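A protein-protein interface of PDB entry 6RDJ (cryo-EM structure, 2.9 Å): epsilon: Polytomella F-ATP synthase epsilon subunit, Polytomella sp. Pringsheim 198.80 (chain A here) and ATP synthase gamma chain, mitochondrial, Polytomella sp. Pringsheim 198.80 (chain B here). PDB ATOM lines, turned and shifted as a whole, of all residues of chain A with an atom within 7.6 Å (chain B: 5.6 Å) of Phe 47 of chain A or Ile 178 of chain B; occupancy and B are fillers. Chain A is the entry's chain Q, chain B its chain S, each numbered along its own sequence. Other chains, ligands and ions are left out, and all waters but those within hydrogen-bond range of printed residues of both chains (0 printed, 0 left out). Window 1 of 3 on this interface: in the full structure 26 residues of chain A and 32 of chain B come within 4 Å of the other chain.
N of Gln 49 of chain A sits at hydrogen-bond distance from O of Lys 61 of chain A, at 2.7 Å. NE2 of Gln 49 of chain A sits at hydrogen-bond distance from OH of Tyr 63 of chain A (3.1 Å). The backbone carbonyl oxygen of Phe 47 of chain A is in hydrogen-bond range of the backbone NH of Tyr 63 of chain A (3.1 Å). OG1 of Thr 165 of chain B sits at hydrogen-bond distance from SD of Met 259 of chain B (3.5 Å). The backbone carbonyl oxygen (O) of Leu 65 of chain A lies within hydrogen-bond range of the backbone NH (N) of Ile 45 of chain A. NZ of Lys 61 of chain A is in hydrogen-bond range of OH of Tyr 63 of chain A.
Leu 17 of chain A touches Ser 176 of chain B (CD1 to O, 3.9 Å). Leu 17 of chain A touches Val 179 of chain B. Ile 45 of chain A touches Gly 173 of chain B. N of Gln 174 of chain B touches CG1 of Ile 45 of chain A, at 3.8 Å. Leu 177 of chain B touches Ile 45 of chain A (CD1 to CD1, 3.8 Å). Phe 47 of chain A touches Ile 162 of chain B. Asp 164 of chain B touches Phe 47 of chain A (O to CA, 3.8 Å). CG of Gln 174 of chain B touches CD1 of Phe 47 of chain A, at 3.8 Å. Phe 47 of chain A touches Leu 177 of chain B. O of Arg 48 of chain A touches CA of Ile 162 of chain B, 3.4 Å away.
Of the printed residues of chain B, Ile 45 of chain A touches Gly 173, Gln 174 and Leu 177. Of the printed residues of chain B, Gln 49 of chain A touches Glu 181. Printed residues of chain A within 4 Å of Ser 176 of chain B: Leu 17 (3.9 Å). Ile 178 of chain B touches one residue of chain A. Of the printed residues of chain A, Glu 181 of chain B touches Gln 49. The nearest residue of chain A that does not touch Ile 178 of chain B is Gln 49 of chain A (6.6 Å). The nearest printed residue of chain A that does not touch Asp 164 of chain B is Val 62 of chain A (6.1 Å).
Hydrophobic or aromatic side chains of chain B within 4 Å of the printed part of chain A: Ile 162, Ala 163, Leu 177, Ile 178 and Val 179. Among the printed residues, 20 pairs touch across the chains. Among the printed residues, Asp or Glu carboxylates within 4 Å of a Lys or Arg side-chain nitrogen of the other chain: Arg 48 of chain A with Asp 164 of chain B (2.9 Å).
N of Ala 163 of chain B sits at hydrogen-bond distance from O of Arg 48 of chain A (3.0 Å). The backbone carbonyl oxygen of His 46 of chain A sits at hydrogen-bond distance from the side-chain amide nitrogen of Gln 174 of chain B, 2.9 Å away. The backbone carbonyl oxygen (O) of His 46 of chain A lies close to the backbone carbonyl oxygen (O) of Asp 164 of chain B, at 3.2 Å. The guanidinium group of Arg 48 of chain A lies within salt-bridge range of the side-chain carboxylate of Asp 164 of chain B.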
ATOM      1  N   LEU A  17      19.340   1.835 -19.763  1.00  0.00           N
ATOM      2  CA  LEU A  17      18.820   0.488 -19.961  1.00  0.00           C
ATOM      3  C   LEU A  17      17.924   0.413 -21.179  1.00  0.00           C
ATOM      4  O   LEU A  17      18.037  -0.520 -21.979  1.00  0.00           O
ATOM      5  CB  LEU A  17      18.046   0.044 -18.732  1.00  0.00           C
ATOM      6  CG  LEU A  17      18.874  -0.413 -17.553  1.00  0.00           C
ATOM      7  CD1 LEU A  17      17.945  -0.513 -16.405  1.00  0.00           C
ATOM      8  CD2 LEU A  17      19.478  -1.750 -17.866  1.00  0.00           C
ATOM      9  N   ALA A  44      11.119 -10.895 -25.763  1.00  0.00           N
ATOM     10  CA  ALA A  44       9.751 -10.666 -25.332  1.00  0.00           C
ATOM     11  C   ALA A  44       9.696 -10.193 -23.889  1.00  0.00           C
ATOM     12  O   ALA A  44      10.474 -10.622 -23.039  1.00  0.00           O
ATOM     13  CB  ALA A  44       8.922 -11.938 -25.484  1.00  0.00           C
ATOM     14  N   ILE A  45       8.749  -9.305 -23.619  1.00  0.00           N
ATOM     15  CA  ILE A  45       8.549  -8.739 -22.291  1.00  0.00           C
ATOM     16  C   ILE A  45       7.136  -9.075 -21.858  1.00  0.00           C
ATOM     17  O   ILE A  45       6.169  -8.628 -22.484  1.00  0.00           O
ATOM     18  CB  ILE A  45       8.775  -7.222 -22.276  1.00  0.00           C
ATOM     19  CG1 ILE A  45      10.217  -6.903 -22.651  1.00  0.00           C
ATOM     20  CG2 ILE A  45       8.443  -6.660 -20.915  1.00  0.00           C
ATOM     21  CD1 ILE A  45      10.491  -5.441 -22.736  1.00  0.00           C
ATOM     22  N   HIS A  46       7.014  -9.853 -20.788  1.00  0.00           N
ATOM     23  CA  HIS A  46       5.715 -10.335 -20.316  1.00  0.00           C
ATOM     24  C   HIS A  46       5.697 -10.244 -18.795  1.00  0.00           C
ATOM     25  O   HIS A  46       6.188 -11.144 -18.111  1.00  0.00           O
ATOM     26  CB  HIS A  46       5.457 -11.758 -20.785  1.00  0.00           C
ATOM     27  CG  HIS A  46       5.134 -11.875 -22.239  1.00  0.00           C
ATOM     28  ND1 HIS A  46       5.908 -12.602 -23.117  1.00  0.00           N
ATOM     29  CD2 HIS A  46       4.109 -11.376 -22.965  1.00  0.00           C
ATOM     30  CE1 HIS A  46       5.378 -12.538 -24.324  1.00  0.00           C
ATOM     31  NE2 HIS A  46       4.286 -11.800 -24.260  1.00  0.00           N
ATOM     32  N   PHE A  47       5.119  -9.168 -18.276  1.00  0.00           N
ATOM     33  CA  PHE A  47       4.876  -9.037 -16.846  1.00  0.00           C
ATOM     34  C   PHE A  47       3.733  -8.053 -16.652  1.00  0.00           C
ATOM     35  O   PHE A  47       3.055  -7.672 -17.609  1.00  0.00           O
ATOM     36  CB  PHE A  47       6.151  -8.632 -16.088  1.00  0.00           C
ATOM     37  CG  PHE A  47       6.554  -7.194 -16.254  1.00  0.00           C
ATOM     38  CD1 PHE A  47       7.097  -6.741 -17.443  1.00  0.00           C
ATOM     39  CD2 PHE A  47       6.449  -6.312 -15.195  1.00  0.00           C
ATOM     40  CE1 PHE A  47       7.484  -5.432 -17.583  1.00  0.00           C
ATOM     41  CE2 PHE A  47       6.838  -5.003 -15.329  1.00  0.00           C
ATOM     42  CZ  PHE A  47       7.357  -4.563 -16.522  1.00  0.00           C
ATOM     43  N   ARG A  48       3.489  -7.678 -15.404  1.00  0.00           N
ATOM     44  CA  ARG A  48       2.477  -6.689 -15.080  1.00  0.00           C
ATOM     45  C   ARG A  48       2.880  -6.005 -13.785  1.00  0.00           C
ATOM     46  O   ARG A  48       3.675  -6.535 -13.005  1.00  0.00           O
ATOM     47  CB  ARG A  48       1.089  -7.324 -14.960  1.00  0.00           C
ATOM     48  CG  ARG A  48       0.822  -7.993 -13.638  1.00  0.00           C
ATOM     49  CD  ARG A  48      -0.639  -8.310 -13.466  1.00  0.00           C
ATOM     50  NE  ARG A  48      -0.992  -8.372 -12.056  1.00  0.00           N
ATOM     51  CZ  ARG A  48      -0.945  -9.479 -11.331  1.00  0.00           C
ATOM     52  NH1 ARG A  48      -1.275  -9.448 -10.049  1.00  0.00           N
ATOM     53  NH2 ARG A  48      -0.563 -10.616 -11.886  1.00  0.00           N
ATOM     54  N   GLN A  49       2.340  -4.811 -13.561  1.00  0.00           N
ATOM     55  CA  GLN A  49       2.748  -4.048 -12.393  1.00  0.00           C
ATOM     56  C   GLN A  49       1.610  -3.164 -11.919  1.00  0.00           C
ATOM     57  O   GLN A  49       0.694  -2.831 -12.674  1.00  0.00           O
ATOM     58  CB  GLN A  49       3.986  -3.203 -12.676  1.00  0.00           C
ATOM     59  CG  GLN A  49       3.913  -2.418 -13.956  1.00  0.00           C
ATOM     60  CD  GLN A  49       4.758  -1.181 -13.895  1.00  0.00           C
ATOM     61  OE1 GLN A  49       4.974  -0.624 -12.824  1.00  0.00           O
ATOM     62  NE2 GLN A  49       5.242  -0.738 -15.043  1.00  0.00           N
ATOM     63  N   ALA A  50       1.695  -2.774 -10.654  1.00  0.00           N
ATOM     64  CA  ALA A  50       0.620  -2.069  -9.977  1.00  0.00           C
ATOM     65  C   ALA A  50       1.158  -1.308  -8.774  1.00  0.00           C
ATOM     66  O   ALA A  50       1.776  -1.914  -7.891  1.00  0.00           O
ATOM     67  CB  ALA A  50      -0.454  -3.059  -9.535  1.00  0.00           C
ATOM     68  N   LYS A  61      -1.103  -2.104 -14.651  1.00  0.00           N
ATOM     69  CA  LYS A  61      -0.355  -1.854 -15.876  1.00  0.00           C
ATOM     70  C   LYS A  61       0.192  -3.194 -16.335  1.00  0.00           C
ATOM     71  O   LYS A  61       0.709  -3.954 -15.514  1.00  0.00           O
ATOM     72  CB  LYS A  61       0.773  -0.845 -15.635  1.00  0.00           C
ATOM     73  CG  LYS A  61       1.704  -0.637 -16.810  1.00  0.00           C
ATOM     74  CD  LYS A  61       0.948  -0.177 -18.039  1.00  0.00           C
ATOM     75  CE  LYS A  61       1.858  -0.071 -19.241  1.00  0.00           C
ATOM     76  NZ  LYS A  61       2.901   0.957 -19.035  1.00  0.00           N
ATOM     77  N   VAL A  62       0.069  -3.491 -17.623  1.00  0.00           N
ATOM     78  CA  VAL A  62       0.436  -4.801 -18.147  1.00  0.00           C
ATOM     79  C   VAL A  62       1.285  -4.608 -19.398  1.00  0.00           C
ATOM     80  O   VAL A  62       1.156  -3.602 -20.103  1.00  0.00           O
ATOM     81  CB  VAL A  62      -0.826  -5.661 -18.416  1.00  0.00           C
ATOM     82  CG1 VAL A  62      -1.663  -5.116 -19.571  1.00  0.00           C
ATOM     83  CG2 VAL A  62      -0.487  -7.138 -18.611  1.00  0.00           C
ATOM     84  N   TYR A  63       2.197  -5.548 -19.637  1.00  0.00           N
ATOM     85  CA  TYR A  63       3.107  -5.526 -20.772  1.00  0.00           C
ATOM     86  C   TYR A  63       3.067  -6.891 -21.434  1.00  0.00           C
ATOM     87  O   TYR A  63       3.426  -7.891 -20.810  1.00  0.00           O
ATOM     88  CB  TYR A  63       4.537  -5.213 -20.334  1.00  0.00           C
ATOM     89  CG  TYR A  63       4.745  -3.854 -19.723  1.00  0.00           C
ATOM     90  CD1 TYR A  63       4.532  -3.644 -18.373  1.00  0.00           C
ATOM     91  CD2 TYR A  63       5.190  -2.790 -20.490  1.00  0.00           C
ATOM     92  CE1 TYR A  63       4.735  -2.411 -17.806  1.00  0.00           C
ATOM     93  CE2 TYR A  63       5.396  -1.550 -19.932  1.00  0.00           C
ATOM     94  CZ  TYR A  63       5.167  -1.365 -18.590  1.00  0.00           C
ATOM     95  OH  TYR A  63       5.373  -0.128 -18.031  1.00  0.00           O
ATOM     96  N   GLU A  64       2.638  -6.937 -22.689  1.00  0.00           N
ATOM     97  CA  GLU A  64       2.618  -8.200 -23.413  1.00  0.00           C
ATOM     98  C   GLU A  64       3.348  -8.032 -24.731  1.00  0.00           C
ATOM     99  O   GLU A  64       2.857  -8.417 -25.796  1.00  0.00           O
ATOM    100  CB  GLU A  64       1.189  -8.699 -23.621  1.00  0.00           C
ATOM    101  CG  GLU A  64       0.537  -9.170 -22.332  1.00  0.00           C
ATOM    102  CD  GLU A  64      -0.845  -9.732 -22.540  1.00  0.00           C
ATOM    103  OE1 GLU A  64      -1.365  -9.635 -23.671  1.00  0.00           O
ATOM    104  OE2 GLU A  64      -1.405 -10.281 -21.568  1.00  0.00           O
ATOM    105  N   LEU A  65       4.530  -7.442 -24.647  1.00  0.00           N
ATOM    106  CA  LEU A  65       5.336  -7.117 -25.806  1.00  0.00           C
ATOM    107  C   LEU A  65       6.150  -8.341 -26.196  1.00  0.00           C
ATOM    108  O   LEU A  65       6.953  -8.834 -25.400  1.00  0.00           O
ATOM    109  CB  LEU A  65       6.245  -5.943 -25.463  1.00  0.00           C
ATOM    110  CG  LEU A  65       5.411  -4.752 -25.004  1.00  0.00           C
ATOM    111  CD1 LEU A  65       6.279  -3.689 -24.377  1.00  0.00           C
ATOM    112  CD2 LEU A  65       4.618  -4.194 -26.174  1.00  0.00           C
ATOM    113  N   ILE B 142       8.498  -8.563  -6.332  1.00  0.00           N
ATOM    114  CA  ILE B 142       8.435  -9.180  -7.648  1.00  0.00           C
ATOM    115  C   ILE B 142       7.816 -10.557  -7.466  1.00  0.00           C
ATOM    116  O   ILE B 142       8.426 -11.448  -6.869  1.00  0.00           O
ATOM    117  CB  ILE B 142       9.814  -9.257  -8.311  1.00  0.00           C
ATOM    118  CG1 ILE B 142      10.319  -7.850  -8.607  1.00  0.00           C
ATOM    119  CG2 ILE B 142       9.733 -10.056  -9.583  1.00  0.00           C
ATOM    120  CD1 ILE B 142      11.622  -7.808  -9.324  1.00  0.00           C
ATOM    121  N   ILE B 162       5.183  -5.931  -8.765  1.00  0.00           N
ATOM    122  CA  ILE B 162       5.412  -6.578 -10.051  1.00  0.00           C
ATOM    123  C   ILE B 162       5.012  -8.038  -9.921  1.00  0.00           C
ATOM    124  O   ILE B 162       5.409  -8.715  -8.968  1.00  0.00           O
ATOM    125  CB  ILE B 162       6.878  -6.443 -10.499  1.00  0.00           C
ATOM    126  CG1 ILE B 162       7.240  -4.995 -10.802  1.00  0.00           C
ATOM    127  CG2 ILE B 162       7.150  -7.253 -11.735  1.00  0.00           C
ATOM    128  CD1 ILE B 162       7.968  -4.307  -9.708  1.00  0.00           C
ATOM    129  N   ALA B 163       4.215  -8.521 -10.867  1.00  0.00           N
ATOM    130  CA  ALA B 163       3.777  -9.900 -10.872  1.00  0.00           C
ATOM    131  C   ALA B 163       3.775 -10.405 -12.305  1.00  0.00           C
ATOM    132  O   ALA B 163       4.116  -9.675 -13.236  1.00  0.00           O
ATOM    133  CB  ALA B 163       2.398 -10.028 -10.229  1.00  0.00           C
ATOM    134  N   ASP B 164       3.399 -11.677 -12.462  1.00  0.00           N
ATOM    135  CA  ASP B 164       3.285 -12.393 -13.734  1.00  0.00           C
ATOM    136  C   ASP B 164       4.591 -12.445 -14.515  1.00  0.00           C
ATOM    137  O   ASP B 164       4.574 -12.620 -15.734  1.00  0.00           O
ATOM    138  CB  ASP B 164       2.176 -11.808 -14.618  1.00  0.00           C
ATOM    139  CG  ASP B 164       0.800 -12.331 -14.256  1.00  0.00           C
ATOM    140  OD1 ASP B 164      -0.200 -11.665 -14.598  1.00  0.00           O
ATOM    141  OD2 ASP B 164       0.717 -13.407 -13.626  1.00  0.00           O
ATOM    142  N   THR B 165       5.731 -12.329 -13.843  1.00  0.00           N
ATOM    143  CA  THR B 165       6.991 -12.162 -14.552  1.00  0.00           C
ATOM    144  C   THR B 165       7.583 -13.467 -15.055  1.00  0.00           C
ATOM    145  O   THR B 165       8.236 -13.469 -16.101  1.00  0.00           O
ATOM    146  CB  THR B 165       8.007 -11.445 -13.665  1.00  0.00           C
ATOM    147  OG1 THR B 165       9.310 -11.591 -14.230  1.00  0.00           O
ATOM    148  CG2 THR B 165       7.992 -11.998 -12.269  1.00  0.00           C
ATOM    149  N   GLY B 173      15.089  -7.445 -21.094  1.00  0.00           N
ATOM    150  CA  GLY B 173      14.243  -6.286 -21.314  1.00  0.00           C
ATOM    151  C   GLY B 173      13.174  -6.144 -20.254  1.00  0.00           C
ATOM    152  O   GLY B 173      12.812  -5.029 -19.871  1.00  0.00           O
ATOM    153  N   GLN B 174      12.699  -7.269 -19.734  1.00  0.00           N
ATOM    154  CA  GLN B 174      11.722  -7.267 -18.656  1.00  0.00           C
ATOM    155  C   GLN B 174      12.331  -6.745 -17.363  1.00  0.00           C
ATOM    156  O   GLN B 174      11.746  -5.888 -16.688  1.00  0.00           O
ATOM    157  CB  GLN B 174      11.197  -8.684 -18.490  1.00  0.00           C
ATOM    158  CG  GLN B 174      10.261  -8.912 -17.370  1.00  0.00           C
ATOM    159  CD  GLN B 174       9.939 -10.363 -17.271  1.00  0.00           C
ATOM    160  OE1 GLN B 174      10.485 -11.071 -16.434  1.00  0.00           O
ATOM    161  NE2 GLN B 174       9.079 -10.836 -18.153  1.00  0.00           N
ATOM    162  N   ALA B 175      13.522  -7.238 -17.016  1.00  0.00           N
ATOM    163  CA  ALA B 175      14.231  -6.732 -15.848  1.00  0.00           C
ATOM    164  C   ALA B 175      14.628  -5.277 -16.022  1.00  0.00           C
ATOM    165  O   ALA B 175      14.652  -4.524 -15.047  1.00  0.00           O
ATOM    166  CB  ALA B 175      15.463  -7.584 -15.579  1.00  0.00           C
ATOM    167  N   SER B 176      14.894  -4.859 -17.257  1.00  0.00           N
ATOM    168  CA  SER B 176      15.215  -3.469 -17.539  1.00  0.00           C
ATOM    169  C   SER B 176      14.010  -2.567 -17.333  1.00  0.00           C
ATOM    170  O   SER B 176      14.150  -1.464 -16.800  1.00  0.00           O
ATOM    171  CB  SER B 176      15.733  -3.342 -18.962  1.00  0.00           C
ATOM    172  OG  SER B 176      16.698  -4.334 -19.221  1.00  0.00           O
ATOM    173  N   LEU B 177      12.820  -3.015 -17.741  1.00  0.00           N
ATOM    174  CA  LEU B 177      11.619  -2.216 -17.508  1.00  0.00           C
ATOM    175  C   LEU B 177      11.279  -2.141 -16.026  1.00  0.00           C
ATOM    176  O   LEU B 177      10.840  -1.090 -15.538  1.00  0.00           O
ATOM    177  CB  LEU B 177      10.444  -2.795 -18.282  1.00  0.00           C
ATOM    178  CG  LEU B 177      10.376  -2.573 -19.787  1.00  0.00           C
ATOM    179  CD1 LEU B 177       9.017  -2.973 -20.290  1.00  0.00           C
ATOM    180  CD2 LEU B 177      10.653  -1.132 -20.126  1.00  0.00           C
ATOM    181  N   ILE B 178      11.490  -3.236 -15.295  1.00  0.00           N
ATOM    182  CA  ILE B 178      11.273  -3.210 -13.850  1.00  0.00           C
ATOM    183  C   ILE B 178      12.269  -2.276 -13.176  1.00  0.00           C
ATOM    184  O   ILE B 178      11.913  -1.515 -12.268  1.00  0.00           O
ATOM    185  CB  ILE B 178      11.347  -4.636 -13.279  1.00  0.00           C
ATOM    186  CG1 ILE B 178      10.228  -5.486 -13.853  1.00  0.00           C
ATOM    187  CG2 ILE B 178      11.198  -4.634 -11.786  1.00  0.00           C
ATOM    188  CD1 ILE B 178      10.436  -6.946 -13.643  1.00  0.00           C
ATOM    189  N   VAL B 179      13.515  -2.269 -13.648  1.00  0.00           N
ATOM    190  CA  VAL B 179      14.502  -1.353 -13.100  1.00  0.00           C
ATOM    191  C   VAL B 179      14.192   0.090 -13.459  1.00  0.00           C
ATOM    192  O   VAL B 179      14.458   0.984 -12.656  1.00  0.00           O
ATOM    193  CB  VAL B 179      15.894  -1.733 -13.579  1.00  0.00           C
ATOM    194  N   GLU B 180      13.617   0.333 -14.638  1.00  0.00           N
ATOM    195  CA  GLU B 180      13.176   1.679 -14.998  1.00  0.00           C
ATOM    196  C   GLU B 180      12.087   2.161 -14.057  1.00  0.00           C
ATOM    197  O   GLU B 180      12.095   3.316 -13.617  1.00  0.00           O
ATOM    198  CB  GLU B 180      12.660   1.701 -16.429  1.00  0.00           C
ATOM    199  CG  GLU B 180      13.725   1.728 -17.483  1.00  0.00           C
ATOM    200  CD  GLU B 180      13.144   1.994 -18.847  1.00  0.00           C
ATOM    201  OE1 GLU B 180      12.428   3.004 -19.003  1.00  0.00           O
ATOM    202  OE2 GLU B 180      13.372   1.175 -19.756  1.00  0.00           O
ATOM    203  N   GLU B 181      11.148   1.276 -13.724  1.00  0.00           N
ATOM    204  CA  GLU B 181      10.112   1.633 -12.767  1.00  0.00           C
ATOM    205  C   GLU B 181      10.657   1.805 -11.354  1.00  0.00           C
ATOM    206  O   GLU B 181      10.064   2.538 -10.562  1.00  0.00           O
ATOM    207  CB  GLU B 181       8.999   0.591 -12.790  1.00  0.00           C
ATOM    208  CG  GLU B 181       7.685   1.116 -12.258  1.00  0.00           C
ATOM    209  CD  GLU B 181       7.105   2.238 -13.102  1.00  0.00           C
ATOM    210  OE1 GLU B 181       6.468   3.146 -12.527  1.00  0.00           O
ATOM    211  OE2 GLU B 181       7.268   2.202 -14.342  1.00  0.00           O
ATOM    212  N   LEU B 182      11.770   1.162 -11.019  1.00  0.00           N
ATOM    213  CA  LEU B 182      12.391   1.468  -9.733  1.00  0.00           C
ATOM    214  C   LEU B 182      13.148   2.788  -9.767  1.00  0.00           C
ATOM    215  O   LEU B 182      13.271   3.450  -8.735  1.00  0.00           O
ATOM    216  CB  LEU B 182      13.340   0.353  -9.310  1.00  0.00           C
ATOM    217  CG  LEU B 182      12.716  -1.025  -9.122  1.00  0.00           C
ATOM    218  CD1 LEU B 182      13.752  -1.987  -8.610  1.00  0.00           C
ATOM    219  CD2 LEU B 182      11.541  -0.950  -8.193  1.00  0.00           C
ATOM    220  N   ILE B 183      13.677   3.169 -10.932  1.00  0.00           N
ATOM    221  CA  ILE B 183      14.393   4.435 -11.094  1.00  0.00           C
ATOM    222  C   ILE B 183      13.431   5.605 -11.292  1.00  0.00           C
ATOM    223  O   ILE B 183      13.847   6.770 -11.202  1.00  0.00           O
ATOM    224  CB  ILE B 183      15.444   4.142 -12.190  1.00  0.00           C
ATOM    225  CG1 ILE B 183      16.516   3.229 -11.618  1.00  0.00           C
ATOM    226  CG2 ILE B 183      16.183   5.359 -12.714  1.00  0.00           C
ATOM    227  CD1 ILE B 183      17.361   2.580 -12.656  1.00  0.00           C
ATOM    228  N   LEU B 255      18.901  -7.496 -11.052  1.00  0.00           N
ATOM    229  CA  LEU B 255      17.497  -7.866 -11.016  1.00  0.00           C
ATOM    230  C   LEU B 255      17.213  -9.078 -11.891  1.00  0.00           C
ATOM    231  O   LEU B 255      16.464  -9.974 -11.487  1.00  0.00           O
ATOM    232  CB  LEU B 255      16.684  -6.666 -11.465  1.00  0.00           C
ATOM    233  CG  LEU B 255      15.248  -6.524 -11.044  1.00  0.00           C
ATOM    234  CD1 LEU B 255      15.194  -6.586  -9.551  1.00  0.00           C
ATOM    235  CD2 LEU B 255      14.834  -5.175 -11.514  1.00  0.00           C
ATOM    236  N   MET B 259      15.915 -12.630 -10.233  1.00  0.00           N
ATOM    237  CA  MET B 259      14.708 -13.370 -10.529  1.00  0.00           C
ATOM    238  C   MET B 259      14.941 -14.540 -11.475  1.00  0.00           C
ATOM    239  O   MET B 259      13.980 -15.214 -11.835  1.00  0.00           O
ATOM    240  CB  MET B 259      13.632 -12.433 -11.064  1.00  0.00           C
ATOM    241  CG  MET B 259      13.873 -11.900 -12.407  1.00  0.00           C
ATOM    242  SD  MET B 259      12.477 -10.908 -12.911  1.00  0.00           S
ATOM    243  CE  MET B 259      13.070  -9.313 -12.425  1.00  0.00           C
